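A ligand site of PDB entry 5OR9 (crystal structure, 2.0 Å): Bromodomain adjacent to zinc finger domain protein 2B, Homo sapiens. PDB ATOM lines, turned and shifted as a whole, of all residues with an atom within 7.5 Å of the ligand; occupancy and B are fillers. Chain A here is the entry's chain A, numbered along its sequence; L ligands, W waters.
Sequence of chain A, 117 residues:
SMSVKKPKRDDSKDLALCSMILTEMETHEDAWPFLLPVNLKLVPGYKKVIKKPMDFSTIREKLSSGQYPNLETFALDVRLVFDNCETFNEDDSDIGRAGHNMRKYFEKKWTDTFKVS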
ATOM      1  N   ALA A  31      17.429   7.628  -3.193  1.00  0.00           N
ATOM      2  CA  ALA A  31      18.174   8.834  -2.874  1.00  0.00           C
ATOM      3  C   ALA A  31      17.540   9.665  -1.761  1.00  0.00           C
ATOM      4  O   ALA A  31      18.202  10.578  -1.244  1.00  0.00           O
ATOM      5  CB  ALA A  31      18.323   9.723  -4.117  1.00  0.00           C
ATOM      6  N   TRP A  32      16.302   9.381  -1.383  1.00  0.00           N
ATOM      7  CA  TRP A  32      15.591  10.266  -0.465  1.00  0.00           C
ATOM      8  C   TRP A  32      16.311  10.533   0.851  1.00  0.00           C
ATOM      9  O   TRP A  32      16.158  11.654   1.378  1.00  0.00           O
ATOM     10  CB  TRP A  32      14.183   9.723  -0.206  1.00  0.00           C
ATOM     11  CG  TRP A  32      14.167   8.341   0.341  1.00  0.00           C
ATOM     12  CD1 TRP A  32      14.077   7.182  -0.386  1.00  0.00           C
ATOM     13  CD2 TRP A  32      14.226   7.949   1.723  1.00  0.00           C
ATOM     14  NE1 TRP A  32      14.093   6.099   0.457  1.00  0.00           N
ATOM     15  CE2 TRP A  32      14.185   6.541   1.757  1.00  0.00           C
ATOM     16  CE3 TRP A  32      14.324   8.645   2.923  1.00  0.00           C
ATOM     17  CZ2 TRP A  32      14.228   5.818   2.941  1.00  0.00           C
ATOM     18  CZ3 TRP A  32      14.372   7.941   4.108  1.00  0.00           C
ATOM     19  CH2 TRP A  32      14.319   6.529   4.112  1.00  0.00           C
ATOM     20  N   PRO A  33      17.113   9.629   1.445  1.00  0.00           N
ATOM     21  CA  PRO A  33      17.794  10.003   2.699  1.00  0.00           C
ATOM     22  C   PRO A  33      18.897  11.020   2.495  1.00  0.00           C
ATOM     23  O   PRO A  33      19.362  11.603   3.479  1.00  0.00           O
ATOM     24  CB  PRO A  33      18.367   8.677   3.212  1.00  0.00           C
ATOM     25  CG  PRO A  33      17.676   7.597   2.421  1.00  0.00           C
ATOM     26  CD  PRO A  33      17.420   8.230   1.083  1.00  0.00           C
ATOM     27  N   PHE A  34      19.335  11.228   1.251  1.00  0.00           N
ATOM     28  CA  PHE A  34      20.579  11.948   0.970  1.00  0.00           C
ATOM     29  C   PHE A  34      20.371  13.210   0.145  1.00  0.00           C
ATOM     30  O   PHE A  34      21.364  13.844  -0.230  1.00  0.00           O
ATOM     31  CB  PHE A  34      21.552  11.014   0.244  1.00  0.00           C
ATOM     32  CG  PHE A  34      21.642   9.631   0.870  1.00  0.00           C
ATOM     33  CD1 PHE A  34      22.245   9.468   2.111  1.00  0.00           C
ATOM     34  CD2 PHE A  34      21.114   8.520   0.234  1.00  0.00           C
ATOM     35  CE1 PHE A  34      22.314   8.215   2.718  1.00  0.00           C
ATOM     36  CE2 PHE A  34      21.181   7.259   0.831  1.00  0.00           C
ATOM     37  CZ  PHE A  34      21.786   7.106   2.063  1.00  0.00           C
ATOM     38  N   LEU A  35      19.121  13.581  -0.156  1.00  0.00           N
ATOM     39  CA  LEU A  35      18.881  14.720  -1.020  1.00  0.00           C
ATOM     40  C   LEU A  35      19.094  16.045  -0.291  1.00  0.00           C
ATOM     41  O   LEU A  35      19.436  17.045  -0.926  1.00  0.00           O
ATOM     42  CB  LEU A  35      17.468  14.668  -1.604  1.00  0.00           C
ATOM     43  CG  LEU A  35      17.187  13.524  -2.588  1.00  0.00           C
ATOM     44  CD1 LEU A  35      15.725  13.500  -2.988  1.00  0.00           C
ATOM     45  CD2 LEU A  35      18.086  13.680  -3.814  1.00  0.00           C
ATOM     46  N   LEU A  36      18.911  16.068   1.028  1.00  0.00           N
ATOM     47  CA  LEU A  36      19.014  17.269   1.849  1.00  0.00           C
ATOM     48  C   LEU A  36      19.920  17.005   3.037  1.00  0.00           C
ATOM     49  O   LEU A  36      20.109  15.853   3.430  1.00  0.00           O
ATOM     50  CB  LEU A  36      17.624  17.702   2.359  1.00  0.00           C
ATOM     51  CG  LEU A  36      16.570  18.093   1.335  1.00  0.00           C
ATOM     52  CD1 LEU A  36      15.340  18.604   2.060  1.00  0.00           C
ATOM     53  CD2 LEU A  36      17.110  19.151   0.390  1.00  0.00           C
ATOM     54  N   PRO A  37      20.463  18.052   3.647  1.00  0.00           N
ATOM     55  CA  PRO A  37      21.279  17.840   4.851  1.00  0.00           C
ATOM     56  C   PRO A  37      20.461  17.188   5.954  1.00  0.00           C
ATOM     57  O   PRO A  37      19.264  17.448   6.105  1.00  0.00           O
ATOM     58  CB  PRO A  37      21.709  19.262   5.253  1.00  0.00           C
ATOM     59  CG  PRO A  37      21.515  20.086   4.050  1.00  0.00           C
ATOM     60  CD  PRO A  37      20.420  19.468   3.244  1.00  0.00           C
ATOM     61  N   VAL A  38      21.115  16.326   6.735  1.00  0.00           N
ATOM     62  CA  VAL A  38      20.493  15.824   7.957  1.00  0.00           C
ATOM     63  C   VAL A  38      20.256  17.006   8.882  1.00  0.00           C
ATOM     64  O   VAL A  38      21.113  17.892   9.002  1.00  0.00           O
ATOM     65  CB  VAL A  38      21.369  14.751   8.627  1.00  0.00           C
ATOM     66  CG1 VAL A  38      20.743  14.263   9.941  1.00  0.00           C
ATOM     67  CG2 VAL A  38      21.606  13.572   7.672  1.00  0.00           C
ATOM     68  N   ASN A  39      19.094  17.044   9.516  1.00  0.00           N
ATOM     69  CA  ASN A  39      18.700  18.191  10.331  1.00  0.00           C
ATOM     70  C   ASN A  39      19.423  18.124  11.678  1.00  0.00           C
ATOM     71  O   ASN A  39      19.003  17.401  12.589  1.00  0.00           O
ATOM     72  CB  ASN A  39      17.180  18.219  10.498  1.00  0.00           C
ATOM     73  CG  ASN A  39      16.688  19.498  11.124  1.00  0.00           C
ATOM     74  OD1 ASN A  39      17.318  20.058  12.014  1.00  0.00           O
ATOM     75  ND2 ASN A  39      15.542  19.981  10.651  1.00  0.00           N
ATOM     76  N   VAL A  43      18.029  15.654  14.968  1.00  0.00           N
ATOM     77  CA  VAL A  43      18.591  14.303  15.037  1.00  0.00           C
ATOM     78  C   VAL A  43      19.593  14.277  16.183  1.00  0.00           C
ATOM     79  O   VAL A  43      20.681  14.877  16.065  1.00  0.00           O
ATOM     80  CB  VAL A  43      19.223  13.881  13.717  1.00  0.00           C
ATOM     81  CG1 VAL A  43      19.769  12.460  13.821  1.00  0.00           C
ATOM     82  CG2 VAL A  43      18.210  13.991  12.589  1.00  0.00           C
ATOM     83  N   PRO A  44      19.300  13.620  17.297  1.00  0.00           N
ATOM     84  CA  PRO A  44      20.256  13.578  18.402  1.00  0.00           C
ATOM     85  C   PRO A  44      21.550  12.903  17.974  1.00  0.00           C
ATOM     86  O   PRO A  44      21.545  11.932  17.211  1.00  0.00           O
ATOM     87  CB  PRO A  44      19.529  12.751  19.479  1.00  0.00           C
ATOM     88  CG  PRO A  44      18.100  12.730  19.079  1.00  0.00           C
ATOM     89  CD  PRO A  44      18.083  12.842  17.583  1.00  0.00           C
ATOM     90  N   TYR A  46      23.844  13.550  15.893  1.00  0.00           N
ATOM     91  CA  TYR A  46      24.415  13.600  14.543  1.00  0.00           C
ATOM     92  C   TYR A  46      25.534  14.624  14.450  1.00  0.00           C
ATOM     93  O   TYR A  46      26.637  14.320  13.975  1.00  0.00           O
ATOM     94  CB  TYR A  46      23.334  13.884  13.511  1.00  0.00           C
ATOM     95  CG  TYR A  46      23.769  13.422  12.130  1.00  0.00           C
ATOM     96  CD1 TYR A  46      24.363  14.307  11.251  1.00  0.00           C
ATOM     97  CD2 TYR A  46      23.640  12.090  11.751  1.00  0.00           C
ATOM     98  CE1 TYR A  46      24.773  13.893   9.996  1.00  0.00           C
ATOM     99  CE2 TYR A  46      24.057  11.664  10.494  1.00  0.00           C
ATOM    100  CZ  TYR A  46      24.637  12.572   9.627  1.00  0.00           C
ATOM    101  OH  TYR A  46      25.061  12.176   8.373  1.00  0.00           O
ATOM    102  N   ILE A  50      29.096  13.042  13.649  1.00  0.00           N
ATOM    103  CA  ILE A  50      29.437  13.092  12.232  1.00  0.00           C
ATOM    104  C   ILE A  50      30.179  14.405  12.008  1.00  0.00           C
ATOM    105  O   ILE A  50      29.581  15.475  11.946  1.00  0.00           O
ATOM    106  CB  ILE A  50      28.202  12.968  11.349  1.00  0.00           C
ATOM    107  CG1 ILE A  50      27.488  11.635  11.611  1.00  0.00           C
ATOM    108  CG2 ILE A  50      28.561  13.145   9.842  1.00  0.00           C
ATOM    109  CD1 ILE A  50      28.349  10.383  11.342  1.00  0.00           C
ATOM    110  N   MET A  54      27.495  15.616   4.876  1.00  0.00           N
ATOM    111  CA  MET A  54      27.491  15.855   3.431  1.00  0.00           C
ATOM    112  C   MET A  54      26.230  15.239   2.858  1.00  0.00           C
ATOM    113  O   MET A  54      25.714  14.258   3.407  1.00  0.00           O
ATOM    114  CB  MET A  54      28.753  15.300   2.762  1.00  0.00           C
ATOM    115  CG  MET A  54      28.863  15.558   1.257  1.00  0.00           C
ATOM    116  SD  MET A  54      28.762  17.328   0.864  1.00  0.00           S
ATOM    117  CE  MET A  54      30.114  17.961   1.858  1.00  0.00           C
ATOM    118  N   ASP A  55      25.750  15.805   1.749  1.00  0.00           N
ATOM    119  CA  ASP A  55      24.516  15.352   1.119  1.00  0.00           C
ATOM    120  C   ASP A  55      24.536  15.783  -0.351  1.00  0.00           C
ATOM    121  O   ASP A  55      25.363  16.585  -0.769  1.00  0.00           O
ATOM    122  CB  ASP A  55      23.286  15.907   1.817  1.00  0.00           C
ATOM    123  CG  ASP A  55      23.136  17.405   1.613  1.00  0.00           C
ATOM    124  OD1 ASP A  55      23.932  18.188   2.177  1.00  0.00           O
ATOM    125  OD2 ASP A  55      22.236  17.800   0.838  1.00  0.00           O
ATOM    126  N   VAL A  81      29.240  10.921   1.929  1.00  0.00           N
ATOM    127  CA  VAL A  81      27.816  10.742   2.198  1.00  0.00           C
ATOM    128  C   VAL A  81      27.536   9.334   2.717  1.00  0.00           C
ATOM    129  O   VAL A  81      26.857   9.141   3.736  1.00  0.00           O
ATOM    130  CB  VAL A  81      26.989  11.045   0.931  1.00  0.00           C
ATOM    131  CG1 VAL A  81      25.540  10.679   1.155  1.00  0.00           C
ATOM    132  CG2 VAL A  81      27.137  12.530   0.501  1.00  0.00           C
ATOM    133  N   ASN A  84      29.354   8.504   6.151  1.00  0.00           N
ATOM    134  CA  ASN A  84      28.535   9.042   7.233  1.00  0.00           C
ATOM    135  C   ASN A  84      27.338   8.136   7.508  1.00  0.00           C
ATOM    136  O   ASN A  84      27.050   7.796   8.649  1.00  0.00           O
ATOM    137  CB  ASN A  84      28.049  10.447   6.896  1.00  0.00           C
ATOM    138  CG  ASN A  84      29.172  11.474   6.893  1.00  0.00           C
ATOM    139  OD1 ASN A  84      30.280  11.216   7.376  1.00  0.00           O
ATOM    140  ND2 ASN A  84      28.879  12.641   6.353  1.00  0.00           N
ATOM    141  N   CYS A  85      26.621   7.755   6.444  1.00  0.00           N
ATOM    142  CA  CYS A  85      25.435   6.920   6.575  1.00  0.00           C
ATOM    143  C   CYS A  85      25.771   5.605   7.273  1.00  0.00           C
ATOM    144  O   CYS A  85      24.994   5.119   8.118  1.00  0.00           O
ATOM    145  CB  CYS A  85      24.838   6.658   5.198  1.00  0.00           C
ATOM    146  SG  CYS A  85      23.285   5.727   5.195  1.00  0.00           S
ATOM    147  N   GLU A  86      26.925   5.019   6.944  1.00  0.00           N
ATOM    148  CA  GLU A  86      27.268   3.714   7.503  1.00  0.00           C
ATOM    149  C   GLU A  86      27.752   3.843   8.931  1.00  0.00           C
ATOM    150  O   GLU A  86      27.669   2.874   9.694  1.00  0.00           O
ATOM    151  CB  GLU A  86      28.343   3.055   6.628  1.00  0.00           C
ATOM    152  CG  GLU A  86      28.554   1.590   6.874  1.00  0.00           C
ATOM    153  CD  GLU A  86      29.376   0.940   5.773  1.00  0.00           C
ATOM    154  OE1 GLU A  86      29.585   1.581   4.719  1.00  0.00           O
ATOM    155  OE2 GLU A  86      29.819  -0.195   5.962  1.00  0.00           O
ATOM    156  N   PHE A  88      26.358   6.056  11.104  1.00  0.00           N
ATOM    157  CA  PHE A  88      25.244   6.426  11.966  1.00  0.00           C
ATOM    158  C   PHE A  88      24.063   5.471  11.886  1.00  0.00           C
ATOM    159  O   PHE A  88      23.310   5.361  12.862  1.00  0.00           O
ATOM    160  CB  PHE A  88      24.760   7.840  11.640  1.00  0.00           C
ATOM    161  CG  PHE A  88      24.143   8.558  12.823  1.00  0.00           C
ATOM    162  CD1 PHE A  88      24.947   9.141  13.792  1.00  0.00           C
ATOM    163  CD2 PHE A  88      22.766   8.677  12.956  1.00  0.00           C
ATOM    164  CE1 PHE A  88      24.394   9.799  14.880  1.00  0.00           C
ATOM    165  CE2 PHE A  88      22.205   9.349  14.025  1.00  0.00           C
ATOM    166  CZ  PHE A  88      23.012   9.900  15.001  1.00  0.00           C
ATOM    167  N   ASN A  89      23.872   4.759  10.786  1.00  0.00           N
ATOM    168  CA  ASN A  89      22.671   3.953  10.587  1.00  0.00           C
ATOM    169  C   ASN A  89      22.990   2.461  10.579  1.00  0.00           C
ATOM    170  O   ASN A  89      24.045   2.046  10.085  1.00  0.00           O
ATOM    171  CB  ASN A  89      21.959   4.313   9.284  1.00  0.00           C
ATOM    172  CG  ASN A  89      21.560   5.778   9.222  1.00  0.00           C
ATOM    173  OD1 ASN A  89      20.509   6.172   9.703  1.00  0.00           O
ATOM    174  ND2 ASN A  89      22.403   6.592   8.593  1.00  0.00           N
ATOM    175  N   ILE A  95      17.371   3.634   5.950  1.00  0.00           N
ATOM    176  CA  ILE A  95      18.418   4.577   5.540  1.00  0.00           C
ATOM    177  C   ILE A  95      19.740   3.856   5.348  1.00  0.00           C
ATOM    178  O   ILE A  95      20.473   4.134   4.396  1.00  0.00           O
ATOM    179  CB  ILE A  95      18.535   5.716   6.566  1.00  0.00           C
ATOM    180  CG1 ILE A  95      17.282   6.583   6.538  1.00  0.00           C
ATOM    181  CG2 ILE A  95      19.796   6.544   6.303  1.00  0.00           C
ATOM    182  CD1 ILE A  95      17.264   7.668   7.612  1.00  0.00           C
ATOM    183  N   GLY A  96      20.061   2.922   6.238  1.00  0.00           N
ATOM    184  CA  GLY A  96      21.321   2.190   6.117  1.00  0.00           C
ATOM    185  C   GLY A  96      21.429   1.377   4.843  1.00  0.00           C
ATOM    186  O   GLY A  96      22.464   1.373   4.174  1.00  0.00           O
HETATM  187  C1  LIG L   1      21.544  10.261   5.601  1.00  0.00           C
HETATM  188  C2  LIG L   1      20.537   9.788   9.080  1.00  0.00           C
HETATM  189  C3  LIG L   1      19.423  10.491   8.595  1.00  0.00           C
HETATM  190  C4  LIG L   1      19.667  10.723   7.255  1.00  0.00           C
HETATM  191  C5  LIG L   1      17.866  12.486   6.588  1.00  0.00           C
HETATM  192  C6  LIG L   1      17.156  13.216   5.436  1.00  0.00           C
HETATM  193  C7  LIG L   1      17.725  14.358   5.291  1.00  0.00           C
HETATM  194  C8  LIG L   1      16.609  15.449   5.259  1.00  0.00           C
HETATM  195  C9  LIG L   1      15.318  14.767   5.735  1.00  0.00           C
HETATM  196  C10 LIG L   1      13.256  12.185   4.680  1.00  0.00           C
HETATM  197  C11 LIG L   1      11.936  11.835   4.953  1.00  0.00           C
HETATM  198  C12 LIG L   1      10.994  11.797   3.912  1.00  0.00           C
HETATM  199  C13 LIG L   1      11.395  12.124   2.588  1.00  0.00           C
HETATM  200  C14 LIG L   1      12.727  12.480   2.325  1.00  0.00           C
HETATM  201  C15 LIG L   1      13.658  12.511   3.356  1.00  0.00           C
HETATM  202  C16 LIG L   1      18.395  10.675   9.700  1.00  0.00           C
HETATM  203  C17 LIG L   1      18.832   9.757  10.821  1.00  0.00           C
HETATM  204  C18 LIG L   1      20.310   9.478  10.563  1.00  0.00           C
HETATM  205  F1  LIG L   1      10.453  12.084   1.566  1.00  0.00           F
HETATM  206  N1  LIG L   1      20.913  10.215   6.952  1.00  0.00           N
HETATM  207  N2  LIG L   1      21.431   9.640   8.050  1.00  0.00           N
HETATM  208  N3  LIG L   1      18.830  11.464   6.216  1.00  0.00           N
HETATM  209  N4  LIG L   1      15.588  13.485   5.825  1.00  0.00           N
HETATM  210  O1  LIG L   1      17.668  12.776   7.709  1.00  0.00           O
HETATM  211  O2  LIG L   1      15.222  10.975   6.194  1.00  0.00           O
HETATM  212  O3  LIG L   1      13.860  12.358   7.405  1.00  0.00           O
HETATM  213  S1  LIG L   1      14.500  12.225   6.069  1.00  0.00           S
HETATM  214  O   HOH W   1      17.088  15.129   9.259  1.00  0.00           O
HETATM  215  O   HOH W   2      21.341  13.450   4.294  1.00  0.00           O
HETATM  216  O   HOH W   3      24.144   9.861   7.583  1.00  0.00           O
HETATM  217  O   HOH W   4      24.920  10.234   4.912  1.00  0.00           O
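The backbone carbonyl oxygen of Pro 33 sits at hydrogen-bond distance from a nitrogen (N3) of the ligand. N2 of the ligand lies within hydrogen-bond range of ND2 of Asn 89 (3.2 Å).
The side-chain amide nitrogen (ND2) of Asn 89 is in hydrogen-bond range of the backbone carbonyl oxygen (O) of Cys 85, 3.0 Å away. The backbone carbonyl oxygen of Ile 95 sits at hydrogen-bond distance from the side-chain sulfur of Cys 85 (3.3 Å).
Trp 32 touches the ligand (O to C15, 3.3 Å). CE1 of Phe 34 touches C1 of the ligand (3.6 Å). Leu 36 touches the ligand (O to C7, 3.4 Å). Pro 37 touches the ligand (O to C8, 3.4 Å). Val 38 touches the ligand. Phe 88 touches the ligand. Ile 95 touches the ligand. The nearest printed residue that does not touch the ligand is Tyr 46 (4.1 Å).
Water W3 lies within hydrogen-bond range of the side-chain hydroxyl of Tyr 46 (2.6 Å), a nitrogen (N2) of the ligand (2.8 Å) and the backbone NH of Cys 85 (3.4 Å). Water W1 bridges N of Asn 39 (2.8 Å) and O1 of the ligand (2.9 Å).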
